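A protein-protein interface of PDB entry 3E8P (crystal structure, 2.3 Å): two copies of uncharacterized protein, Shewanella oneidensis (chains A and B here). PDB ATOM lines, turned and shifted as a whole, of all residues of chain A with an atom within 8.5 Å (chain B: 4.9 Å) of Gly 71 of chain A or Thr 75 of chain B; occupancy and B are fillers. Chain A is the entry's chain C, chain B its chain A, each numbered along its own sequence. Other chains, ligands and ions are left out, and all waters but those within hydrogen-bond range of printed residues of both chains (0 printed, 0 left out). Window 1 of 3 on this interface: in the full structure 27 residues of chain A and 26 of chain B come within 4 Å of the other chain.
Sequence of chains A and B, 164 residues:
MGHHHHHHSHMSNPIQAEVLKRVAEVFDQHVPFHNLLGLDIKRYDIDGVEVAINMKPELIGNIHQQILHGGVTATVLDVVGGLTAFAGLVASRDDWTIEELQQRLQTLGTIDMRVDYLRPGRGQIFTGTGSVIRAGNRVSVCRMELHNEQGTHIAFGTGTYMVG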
ATOM      1  N   PHE A  33      17.234  24.001 -33.802  1.00  0.00           N
ATOM      2  CA  PHE A  33      18.012  22.770 -33.706  1.00  0.00           C
ATOM      3  C   PHE A  33      17.198  21.605 -33.153  1.00  0.00           C
ATOM      4  O   PHE A  33      17.450  20.452 -33.501  1.00  0.00           O
ATOM      5  CB  PHE A  33      19.266  22.987 -32.859  1.00  0.00           C
ATOM      6  CG  PHE A  33      20.257  21.851 -32.938  1.00  0.00           C
ATOM      7  CD1 PHE A  33      20.783  21.452 -34.164  1.00  0.00           C
ATOM      8  CD2 PHE A  33      20.690  21.204 -31.783  1.00  0.00           C
ATOM      9  CE1 PHE A  33      21.732  20.419 -34.242  1.00  0.00           C
ATOM     10  CE2 PHE A  33      21.638  20.174 -31.843  1.00  0.00           C
ATOM     11  CZ  PHE A  33      22.160  19.782 -33.075  1.00  0.00           C
ATOM     12  N   LEU A  37      16.512  17.863 -35.123  1.00  0.00           N
ATOM     13  CA  LEU A  37      16.765  16.564 -34.504  1.00  0.00           C
ATOM     14  C   LEU A  37      15.497  15.800 -34.125  1.00  0.00           C
ATOM     15  O   LEU A  37      15.509  14.575 -34.050  1.00  0.00           O
ATOM     16  CB  LEU A  37      17.652  16.737 -33.259  1.00  0.00           C
ATOM     17  CG  LEU A  37      19.179  16.673 -33.444  1.00  0.00           C
ATOM     18  CD1 LEU A  37      19.631  17.617 -34.540  1.00  0.00           C
ATOM     19  CD2 LEU A  37      19.859  17.014 -32.126  1.00  0.00           C
ATOM     20  N   LEU A  39      13.812  16.620 -31.317  1.00  0.00           N
ATOM     21  CA  LEU A  39      13.815  16.654 -29.863  1.00  0.00           C
ATOM     22  C   LEU A  39      12.475  17.179 -29.358  1.00  0.00           C
ATOM     23  O   LEU A  39      12.032  18.251 -29.751  1.00  0.00           O
ATOM     24  CB  LEU A  39      14.968  17.539 -29.371  1.00  0.00           C
ATOM     25  CG  LEU A  39      15.268  17.615 -27.870  1.00  0.00           C
ATOM     26  CD1 LEU A  39      16.689  18.105 -27.651  1.00  0.00           C
ATOM     27  CD2 LEU A  39      14.279  18.540 -27.191  1.00  0.00           C
ATOM     28  N   ILE A  53      13.272  11.597 -27.856  1.00  0.00           N
ATOM     29  CA  ILE A  53      13.667  11.795 -29.231  1.00  0.00           C
ATOM     30  C   ILE A  53      13.624  10.462 -29.948  1.00  0.00           C
ATOM     31  O   ILE A  53      14.195   9.473 -29.492  1.00  0.00           O
ATOM     32  CB  ILE A  53      15.078  12.436 -29.314  1.00  0.00           C
ATOM     33  CG1 ILE A  53      15.454  12.694 -30.773  1.00  0.00           C
ATOM     34  CG2 ILE A  53      16.105  11.553 -28.602  1.00  0.00           C
ATOM     35  CD1 ILE A  53      16.627  13.657 -30.934  1.00  0.00           C
ATOM     36  N   LEU A  59      20.211  10.618 -37.589  1.00  0.00           N
ATOM     37  CA  LEU A  59      20.892  10.694 -36.294  1.00  0.00           C
ATOM     38  C   LEU A  59      21.948   9.613 -36.064  1.00  0.00           C
ATOM     39  O   LEU A  59      22.578   9.577 -35.011  1.00  0.00           O
ATOM     40  CB  LEU A  59      19.869  10.630 -35.159  1.00  0.00           C
ATOM     41  CG  LEU A  59      18.723  11.635 -35.204  1.00  0.00           C
ATOM     42  CD1 LEU A  59      17.811  11.400 -34.015  1.00  0.00           C
ATOM     43  CD2 LEU A  59      19.264  13.047 -35.201  1.00  0.00           C
ATOM     44  N   ILE A  60      22.147   8.734 -37.038  1.00  0.00           N
ATOM     45  CA  ILE A  60      23.123   7.672 -36.884  1.00  0.00           C
ATOM     46  C   ILE A  60      24.547   8.199 -36.967  1.00  0.00           C
ATOM     47  O   ILE A  60      24.861   9.057 -37.796  1.00  0.00           O
ATOM     48  CB  ILE A  60      22.931   6.570 -37.956  1.00  0.00           C
ATOM     49  CG1 ILE A  60      21.789   5.633 -37.550  1.00  0.00           C
ATOM     50  CG2 ILE A  60      24.214   5.767 -38.117  1.00  0.00           C
ATOM     51  CD1 ILE A  60      20.451   6.315 -37.379  1.00  0.00           C
ATOM     52  N   GLY A  61      25.407   7.673 -36.100  1.00  0.00           N
ATOM     53  CA  GLY A  61      26.798   8.080 -36.095  1.00  0.00           C
ATOM     54  C   GLY A  61      27.613   7.123 -36.939  1.00  0.00           C
ATOM     55  O   GLY A  61      28.208   7.510 -37.942  1.00  0.00           O
ATOM     56  N   LEU A  68      23.325   5.561 -32.286  1.00  0.00           N
ATOM     57  CA  LEU A  68      23.047   6.984 -32.147  1.00  0.00           C
ATOM     58  C   LEU A  68      24.352   7.788 -32.074  1.00  0.00           C
ATOM     59  O   LEU A  68      25.292   7.386 -31.396  1.00  0.00           O
ATOM     60  CB  LEU A  68      22.223   7.198 -30.881  1.00  0.00           C
ATOM     61  CG  LEU A  68      21.621   8.566 -30.591  1.00  0.00           C
ATOM     62  CD1 LEU A  68      20.564   8.927 -31.641  1.00  0.00           C
ATOM     63  CD2 LEU A  68      21.004   8.518 -29.207  1.00  0.00           C
ATOM     64  N   HIS A  69      24.412   8.914 -32.781  1.00  0.00           N
ATOM     65  CA  HIS A  69      25.615   9.745 -32.768  1.00  0.00           C
ATOM     66  C   HIS A  69      25.748  10.422 -31.406  1.00  0.00           C
ATOM     67  O   HIS A  69      24.798  11.025 -30.916  1.00  0.00           O
ATOM     68  CB  HIS A  69      25.557  10.807 -33.880  1.00  0.00           C
ATOM     69  CG  HIS A  69      26.852  11.534 -34.091  1.00  0.00           C
ATOM     70  ND1 HIS A  69      27.304  12.524 -33.242  1.00  0.00           N
ATOM     71  CD2 HIS A  69      27.807  11.394 -35.043  1.00  0.00           C
ATOM     72  CE1 HIS A  69      28.480  12.958 -33.659  1.00  0.00           C
ATOM     73  NE2 HIS A  69      28.809  12.290 -34.751  1.00  0.00           N
ATOM     74  N   GLY A  70      26.930  10.314 -30.806  1.00  0.00           N
ATOM     75  CA  GLY A  70      27.168  10.910 -29.501  1.00  0.00           C
ATOM     76  C   GLY A  70      26.747  12.363 -29.394  1.00  0.00           C
ATOM     77  O   GLY A  70      26.372  12.828 -28.318  1.00  0.00           O
ATOM     78  N   GLY A  71      26.804  13.083 -30.507  1.00  0.00           N
ATOM     79  CA  GLY A  71      26.409  14.481 -30.503  1.00  0.00           C
ATOM     80  C   GLY A  71      24.953  14.657 -30.116  1.00  0.00           C
ATOM     81  O   GLY A  71      24.568  15.652 -29.494  1.00  0.00           O
ATOM     82  N   VAL A  72      24.126  13.688 -30.482  1.00  0.00           N
ATOM     83  CA  VAL A  72      22.710  13.768 -30.143  1.00  0.00           C
ATOM     84  C   VAL A  72      22.574  13.600 -28.636  1.00  0.00           C
ATOM     85  O   VAL A  72      21.899  14.384 -27.963  1.00  0.00           O
ATOM     86  CB  VAL A  72      21.916  12.676 -30.860  1.00  0.00           C
ATOM     87  CG1 VAL A  72      20.435  12.784 -30.517  1.00  0.00           C
ATOM     88  CG2 VAL A  72      22.133  12.798 -32.351  1.00  0.00           C
ATOM     89  N   THR A  73      23.239  12.575 -28.115  1.00  0.00           N
ATOM     90  CA  THR A  73      23.232  12.288 -26.679  1.00  0.00           C
ATOM     91  C   THR A  73      23.573  13.539 -25.876  1.00  0.00           C
ATOM     92  O   THR A  73      22.820  13.948 -24.995  1.00  0.00           O
ATOM     93  CB  THR A  73      24.264  11.191 -26.340  1.00  0.00           C
ATOM     94  OG1 THR A  73      23.886   9.969 -26.991  1.00  0.00           O
ATOM     95  CG2 THR A  73      24.340  10.965 -24.829  1.00  0.00           C
ATOM     96  N   ALA A  74      24.706  14.156 -26.193  1.00  0.00           N
ATOM     97  CA  ALA A  74      25.139  15.350 -25.473  1.00  0.00           C
ATOM     98  C   ALA A  74      24.100  16.466 -25.572  1.00  0.00           C
ATOM     99  O   ALA A  74      23.843  17.162 -24.592  1.00  0.00           O
ATOM    100  CB  ALA A  74      26.489  15.831 -26.007  1.00  0.00           C
ATOM    101  N   THR A  75      23.510  16.641 -26.755  1.00  0.00           N
ATOM    102  CA  THR A  75      22.497  17.678 -26.944  1.00  0.00           C
ATOM    103  C   THR A  75      21.312  17.467 -26.010  1.00  0.00           C
ATOM    104  O   THR A  75      20.882  18.386 -25.310  1.00  0.00           O
ATOM    105  CB  THR A  75      21.937  17.688 -28.382  1.00  0.00           C
ATOM    106  OG1 THR A  75      22.984  17.993 -29.312  1.00  0.00           O
ATOM    107  CG2 THR A  75      20.842  18.732 -28.504  1.00  0.00           C
ATOM    108  N   VAL A  76      20.794  16.243 -26.006  1.00  0.00           N
ATOM    109  CA  VAL A  76      19.646  15.893 -25.183  1.00  0.00           C
ATOM    110  C   VAL A  76      19.916  16.069 -23.688  1.00  0.00           C
ATOM    111  O   VAL A  76      19.071  16.605 -22.975  1.00  0.00           O
ATOM    112  CB  VAL A  76      19.170  14.430 -25.487  1.00  0.00           C
ATOM    113  CG1 VAL A  76      17.993  14.051 -24.593  1.00  0.00           C
ATOM    114  CG2 VAL A  76      18.738  14.329 -26.935  1.00  0.00           C
ATOM    115  N   LEU A  77      21.088  15.632 -23.220  1.00  0.00           N
ATOM    116  CA  LEU A  77      21.444  15.756 -21.806  1.00  0.00           C
ATOM    117  C   LEU A  77      21.486  17.222 -21.376  1.00  0.00           C
ATOM    118  O   LEU A  77      20.951  17.584 -20.327  1.00  0.00           O
ATOM    119  CB  LEU A  77      22.800  15.094 -21.530  1.00  0.00           C
ATOM    120  CG  LEU A  77      22.868  13.562 -21.620  1.00  0.00           C
ATOM    121  CD1 LEU A  77      24.313  13.073 -21.494  1.00  0.00           C
ATOM    122  CD2 LEU A  77      21.999  12.959 -20.519  1.00  0.00           C
ATOM    123  N   ASP A  78      22.116  18.059 -22.196  1.00  0.00           N
ATOM    124  CA  ASP A  78      22.234  19.491 -21.926  1.00  0.00           C
ATOM    125  C   ASP A  78      20.873  20.212 -21.832  1.00  0.00           C
ATOM    126  O   ASP A  78      20.672  21.074 -20.974  1.00  0.00           O
ATOM    127  CB  ASP A  78      23.097  20.135 -23.011  1.00  0.00           C
ATOM    128  CG  ASP A  78      23.276  21.619 -22.812  1.00  0.00           C
ATOM    129  OD1 ASP A  78      23.393  22.064 -21.649  1.00  0.00           O
ATOM    130  OD2 ASP A  78      23.318  22.346 -23.827  1.00  0.00           O
ATOM    131  N   MET A 113      29.602  21.292 -18.832  1.00  0.00           N
ATOM    132  CA  MET A 113      28.859  20.046 -18.787  1.00  0.00           C
ATOM    133  C   MET A 113      29.781  18.877 -19.015  1.00  0.00           C
ATOM    134  O   MET A 113      30.716  18.963 -19.808  1.00  0.00           O
ATOM    135  CB  MET A 113      27.757  20.017 -19.857  1.00  0.00           C
ATOM    136  CG  MET A 113      27.106  18.637 -19.986  1.00  0.00           C
ATOM    137  SD  MET A 113      25.668  18.468 -21.303  1.00  0.00           S
ATOM    138  CE  MET A 113      26.712  18.845 -22.898  1.00  0.00           C
ATOM    139  N   VAL A 115      29.732  14.721 -19.908  1.00  0.00           N
ATOM    140  CA  VAL A 115      28.930  13.623 -20.403  1.00  0.00           C
ATOM    141  C   VAL A 115      29.759  12.355 -20.222  1.00  0.00           C
ATOM    142  O   VAL A 115      30.952  12.333 -20.544  1.00  0.00           O
ATOM    143  CB  VAL A 115      28.594  13.794 -21.915  1.00  0.00           C
ATOM    144  CG1 VAL A 115      27.848  12.553 -22.443  1.00  0.00           C
ATOM    145  CG2 VAL A 115      27.737  15.037 -22.123  1.00  0.00           C
ATOM    146  N   TYR A 117      29.702   8.485 -21.374  1.00  0.00           N
ATOM    147  CA  TYR A 117      29.079   7.541 -22.297  1.00  0.00           C
ATOM    148  C   TYR A 117      29.160   6.118 -21.752  1.00  0.00           C
ATOM    149  O   TYR A 117      30.247   5.580 -21.554  1.00  0.00           O
ATOM    150  CB  TYR A 117      29.763   7.627 -23.666  1.00  0.00           C
ATOM    151  CG  TYR A 117      29.629   8.995 -24.296  1.00  0.00           C
ATOM    152  CD1 TYR A 117      30.515  10.021 -23.987  1.00  0.00           C
ATOM    153  CD2 TYR A 117      28.575   9.279 -25.154  1.00  0.00           C
ATOM    154  CE1 TYR A 117      30.350  11.305 -24.521  1.00  0.00           C
ATOM    155  CE2 TYR A 117      28.401  10.551 -25.685  1.00  0.00           C
ATOM    156  CZ  TYR A 117      29.288  11.557 -25.367  1.00  0.00           C
ATOM    157  OH  TYR A 117      29.098  12.813 -25.905  1.00  0.00           O
ATOM    158  N   LEU A 146      20.070   9.628 -19.808  1.00  0.00           N
ATOM    159  CA  LEU A 146      19.420   9.317 -21.079  1.00  0.00           C
ATOM    160  C   LEU A 146      19.333   7.794 -21.187  1.00  0.00           C
ATOM    161  O   LEU A 146      20.310   7.099 -20.915  1.00  0.00           O
ATOM    162  CB  LEU A 146      20.234   9.866 -22.261  1.00  0.00           C
ATOM    163  CG  LEU A 146      19.587   9.736 -23.652  1.00  0.00           C
ATOM    164  CD1 LEU A 146      18.334  10.598 -23.694  1.00  0.00           C
ATOM    165  CD2 LEU A 146      20.549  10.175 -24.752  1.00  0.00           C
ATOM    166  N   PHE B  33      24.709  11.845 -39.207  1.00  0.00           N
ATOM    167  CA  PHE B  33      24.537  13.029 -38.368  1.00  0.00           C
ATOM    168  C   PHE B  33      25.402  14.212 -38.795  1.00  0.00           C
ATOM    169  O   PHE B  33      25.028  15.352 -38.568  1.00  0.00           O
ATOM    170  CB  PHE B  33      24.797  12.708 -36.888  1.00  0.00           C
ATOM    171  CG  PHE B  33      24.317  13.792 -35.943  1.00  0.00           C
ATOM    172  CD1 PHE B  33      23.004  14.261 -36.011  1.00  0.00           C
ATOM    173  CD2 PHE B  33      25.177  14.349 -34.991  1.00  0.00           C
ATOM    174  CE1 PHE B  33      22.549  15.270 -35.149  1.00  0.00           C
ATOM    175  CE2 PHE B  33      24.733  15.361 -34.123  1.00  0.00           C
ATOM    176  CZ  PHE B  33      23.416  15.820 -34.204  1.00  0.00           C
ATOM    177  N   LEU B  37      23.964  17.994 -40.073  1.00  0.00           N
ATOM    178  CA  LEU B  37      24.429  19.272 -39.550  1.00  0.00           C
ATOM    179  C   LEU B  37      25.267  20.059 -40.553  1.00  0.00           C
ATOM    180  O   LEU B  37      25.241  21.287 -40.553  1.00  0.00           O
ATOM    181  CB  LEU B  37      25.244  19.064 -38.260  1.00  0.00           C
ATOM    182  CG  LEU B  37      24.478  19.042 -36.933  1.00  0.00           C
ATOM    183  CD1 LEU B  37      23.383  17.994 -36.987  1.00  0.00           C
ATOM    184  CD2 LEU B  37      25.437  18.745 -35.778  1.00  0.00           C
ATOM    185  N   LEU B  39      28.636  19.163 -40.958  1.00  0.00           N
ATOM    186  CA  LEU B  39      29.966  19.133 -40.363  1.00  0.00           C
ATOM    187  C   LEU B  39      30.999  18.671 -41.400  1.00  0.00           C
ATOM    188  O   LEU B  39      30.818  17.638 -42.041  1.00  0.00           O
ATOM    189  CB  LEU B  39      29.933  18.209 -39.139  1.00  0.00           C
ATOM    190  CG  LEU B  39      31.147  18.060 -38.225  1.00  0.00           C
ATOM    191  CD1 LEU B  39      30.702  17.542 -36.870  1.00  0.00           C
ATOM    192  CD2 LEU B  39      32.142  17.112 -38.856  1.00  0.00           C
ATOM    193  N   GLY B  71      24.320  22.107 -28.318  1.00  0.00           N
ATOM    194  CA  GLY B  71      24.471  20.723 -28.732  1.00  0.00           C
ATOM    195  C   GLY B  71      25.380  20.596 -29.944  1.00  0.00           C
ATOM    196  O   GLY B  71      26.089  19.602 -30.097  1.00  0.00           O
ATOM    197  N   VAL B  72      25.357  21.609 -30.809  1.00  0.00           N
ATOM    198  CA  VAL B  72      26.197  21.608 -31.995  1.00  0.00           C
ATOM    199  C   VAL B  72      27.635  21.794 -31.560  1.00  0.00           C
ATOM    200  O   VAL B  72      28.540  21.103 -32.026  1.00  0.00           O
ATOM    201  CB  VAL B  72      25.849  22.765 -32.949  1.00  0.00           C
ATOM    202  CG1 VAL B  72      26.868  22.816 -34.079  1.00  0.00           C
ATOM    203  CG2 VAL B  72      24.435  22.591 -33.501  1.00  0.00           C
ATOM    204  N   THR B  73      27.844  22.747 -30.664  1.00  0.00           N
ATOM    205  CA  THR B  73      29.188  23.010 -30.163  1.00  0.00           C
ATOM    206  C   THR B  73      29.764  21.730 -29.546  1.00  0.00           C
ATOM    207  O   THR B  73      30.910  21.371 -29.809  1.00  0.00           O
ATOM    208  CB  THR B  73      29.159  24.136 -29.123  1.00  0.00           C
ATOM    209  OG1 THR B  73      28.717  25.346 -29.750  1.00  0.00           O
ATOM    210  CG2 THR B  73      30.529  24.350 -28.537  1.00  0.00           C
ATOM    211  N   ALA B  74      28.956  21.038 -28.750  1.00  0.00           N
ATOM    212  CA  ALA B  74      29.387  19.794 -28.118  1.00  0.00           C
ATOM    213  C   ALA B  74      29.656  18.714 -29.164  1.00  0.00           C
ATOM    214  O   ALA B  74      30.595  17.938 -29.026  1.00  0.00           O
ATOM    215  CB  ALA B  74      28.333  19.316 -27.136  1.00  0.00           C
ATOM    216  N   THR B  75      28.839  18.672 -30.217  1.00  0.00           N
ATOM    217  CA  THR B  75      29.010  17.679 -31.283  1.00  0.00           C
ATOM    218  C   THR B  75      30.355  17.876 -31.986  1.00  0.00           C
ATOM    219  O   THR B  75      31.115  16.919 -32.178  1.00  0.00           O
ATOM    220  CB  THR B  75      27.860  17.770 -32.338  1.00  0.00           C
ATOM    221  OG1 THR B  75      26.620  17.429 -31.713  1.00  0.00           O
ATOM    222  CG2 THR B  75      28.094  16.802 -33.487  1.00  0.00           C
ATOM    223  N   VAL B  76      30.657  19.121 -32.346  1.00  0.00           N
ATOM    224  CA  VAL B  76      31.917  19.435 -33.024  1.00  0.00           C
ATOM    225  C   VAL B  76      33.139  19.140 -32.150  1.00  0.00           C
ATOM    226  O   VAL B  76      34.108  18.542 -32.602  1.00  0.00           O
ATOM    227  CB  VAL B  76      31.974  20.922 -33.448  1.00  0.00           C
ATOM    228  CG1 VAL B  76      33.319  21.227 -34.117  1.00  0.00           C
ATOM    229  CG2 VAL B  76      30.828  21.228 -34.389  1.00  0.00           C
ATOM    230  N   LEU B  77      33.085  19.554 -30.891  1.00  0.00           N
ATOM    231  CA  LEU B  77      34.206  19.327 -29.989  1.00  0.00           C
ATOM    232  C   LEU B  77      34.499  17.842 -29.798  1.00  0.00           C
ATOM    233  O   LEU B  77      35.665  17.447 -29.727  1.00  0.00           O
ATOM    234  CB  LEU B  77      33.941  19.991 -28.635  1.00  0.00           C
ATOM    235  CG  LEU B  77      33.941  21.523 -28.627  1.00  0.00           C
ATOM    236  CD1 LEU B  77      33.374  22.038 -27.308  1.00  0.00           C
ATOM    237  CD2 LEU B  77      35.347  22.029 -28.827  1.00  0.00           C
ATOM    238  N   ASP B  78      33.452  17.020 -29.721  1.00  0.00           N
ATOM    239  CA  ASP B  78      33.623  15.571 -29.532  1.00  0.00           C
ATOM    240  C   ASP B  78      34.266  14.914 -30.753  1.00  0.00           C
ATOM    241  O   ASP B  78      35.165  14.076 -30.625  1.00  0.00           O
ATOM    242  CB  ASP B  78      32.279  14.884 -29.250  1.00  0.00           C
ATOM    243  CG  ASP B  78      32.449  13.421 -28.838  1.00  0.00           C
ATOM    244  OD1 ASP B  78      31.497  12.632 -28.999  1.00  0.00           O
ATOM    245  OD2 ASP B  78      33.538  13.059 -28.338  1.00  0.00           O
ATOM    246  N   VAL B  79      33.799  15.302 -31.934  1.00  0.00           N
ATOM    247  CA  VAL B  79      34.328  14.781 -33.189  1.00  0.00           C
ATOM    248  C   VAL B  79      35.788  15.202 -33.380  1.00  0.00           C
ATOM    249  O   VAL B  79      36.623  14.400 -33.818  1.00  0.00           O
ATOM    250  CB  VAL B  79      33.491  15.285 -34.385  1.00  0.00           C
ATOM    251  CG1 VAL B  79      34.114  14.798 -35.693  1.00  0.00           C
ATOM    252  CG2 VAL B  79      32.046  14.792 -34.246  1.00  0.00           C
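The backbone NH (N) of Phe 33 of chain B lies within hydrogen-bond range of the backbone carbonyl oxygen (O) of Ile 60 of chain A, at 3.1 Å.
ND1 of His 69 of chain A lies within hydrogen-bond range of N of Gly 71 of chain A, 2.8 Å away.
The backbone carbonyl oxygen (O) of Gly 71 of chain A is in hydrogen-bond range of the side-chain hydroxyl (OG1) of Thr 75 of chain A.
The backbone carbonyl oxygen (O) of Gly 71 of chain B is in hydrogen-bond range of the side-chain hydroxyl (OG1) of Thr 75 of chain B, at 2.8 Å.
N of His 69 of chain A sits at hydrogen-bond distance from O of Leu 59 of chain A.
Phe 33 of chain A touches Val 72 of chain B.
Leu 37 of chain A touches Phe 33 of chain B (CD1 to CE1, 3.8 Å).
CE1 of Phe 33 of chain B touches CD2 of Leu 59 of chain A, at 3.97 Å.
ND1 of His 69 of chain A touches CD2 of Phe 33 of chain B (3.3 Å).
His 69 of chain A touches Thr 75 of chain B (CE1 to CG2, 3.9 Å).
Thr 75 of chain B touches Gly 71 of chain A.
Val 72 of chain A touches Phe 33 of chain B.
Gly 71 of chain B touches Thr 75 of chain A.
Asp 78 of chain B touches Tyr 117 of chain A (OD1 to OH, 3.9 Å).
Of chain B, only Thr 75 comes within 4 Å of Gly 71 of chain A.
Thr 75 of chain B touches two residues of chain A.
Of the printed residues of chain B, Phe 33 of chain A touches Val 72 (3.5 Å).
Of the printed residues of chain B, His 69 of chain A touches Phe 33 and Thr 75.
Of the printed residues of chain A, Phe 33 of chain B touches Leu 37, Leu 59, Ile 60, His 69 and Val 72.
Met 113 of chain A touches none of the printed residues of chain B.
Leu 146 of chain A touches none of the printed residues of chain B.
Of the 22 printed residues of chain A, 9 touch a printed residue of chain B.
Hydrophobic or aromatic side chains of chain A within 4 Å of the printed part of chain B: Phe 33, Leu 37, Leu 59, His 69, Val 72 and Tyr 117.
Of the 12 printed residues of chain B, 5 touch a printed residue of chain A.
Printed residues of chain B that touch a printed residue of chain A: Phe 33, Gly 71, Val 72, Thr 75 and Asp 78.
Among the printed residues, 10 pairs touch across the chains.
Phe 33 of chain A touches Val 72 of chain B, and with the chains exchanged Val 72 of chain A touches Phe 33 of chain B.
Leu 37 of chain A touches Phe 33 of chain B, but with the chains exchanged Phe 33 of chain A does not touch Leu 37 of chain B (4.02 Å).
Gly 71 of chain A touches Thr 75 of chain B, and with the chains exchanged Thr 75 of chain A touches Gly 71 of chain B.
11 positions are printed for both chains.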
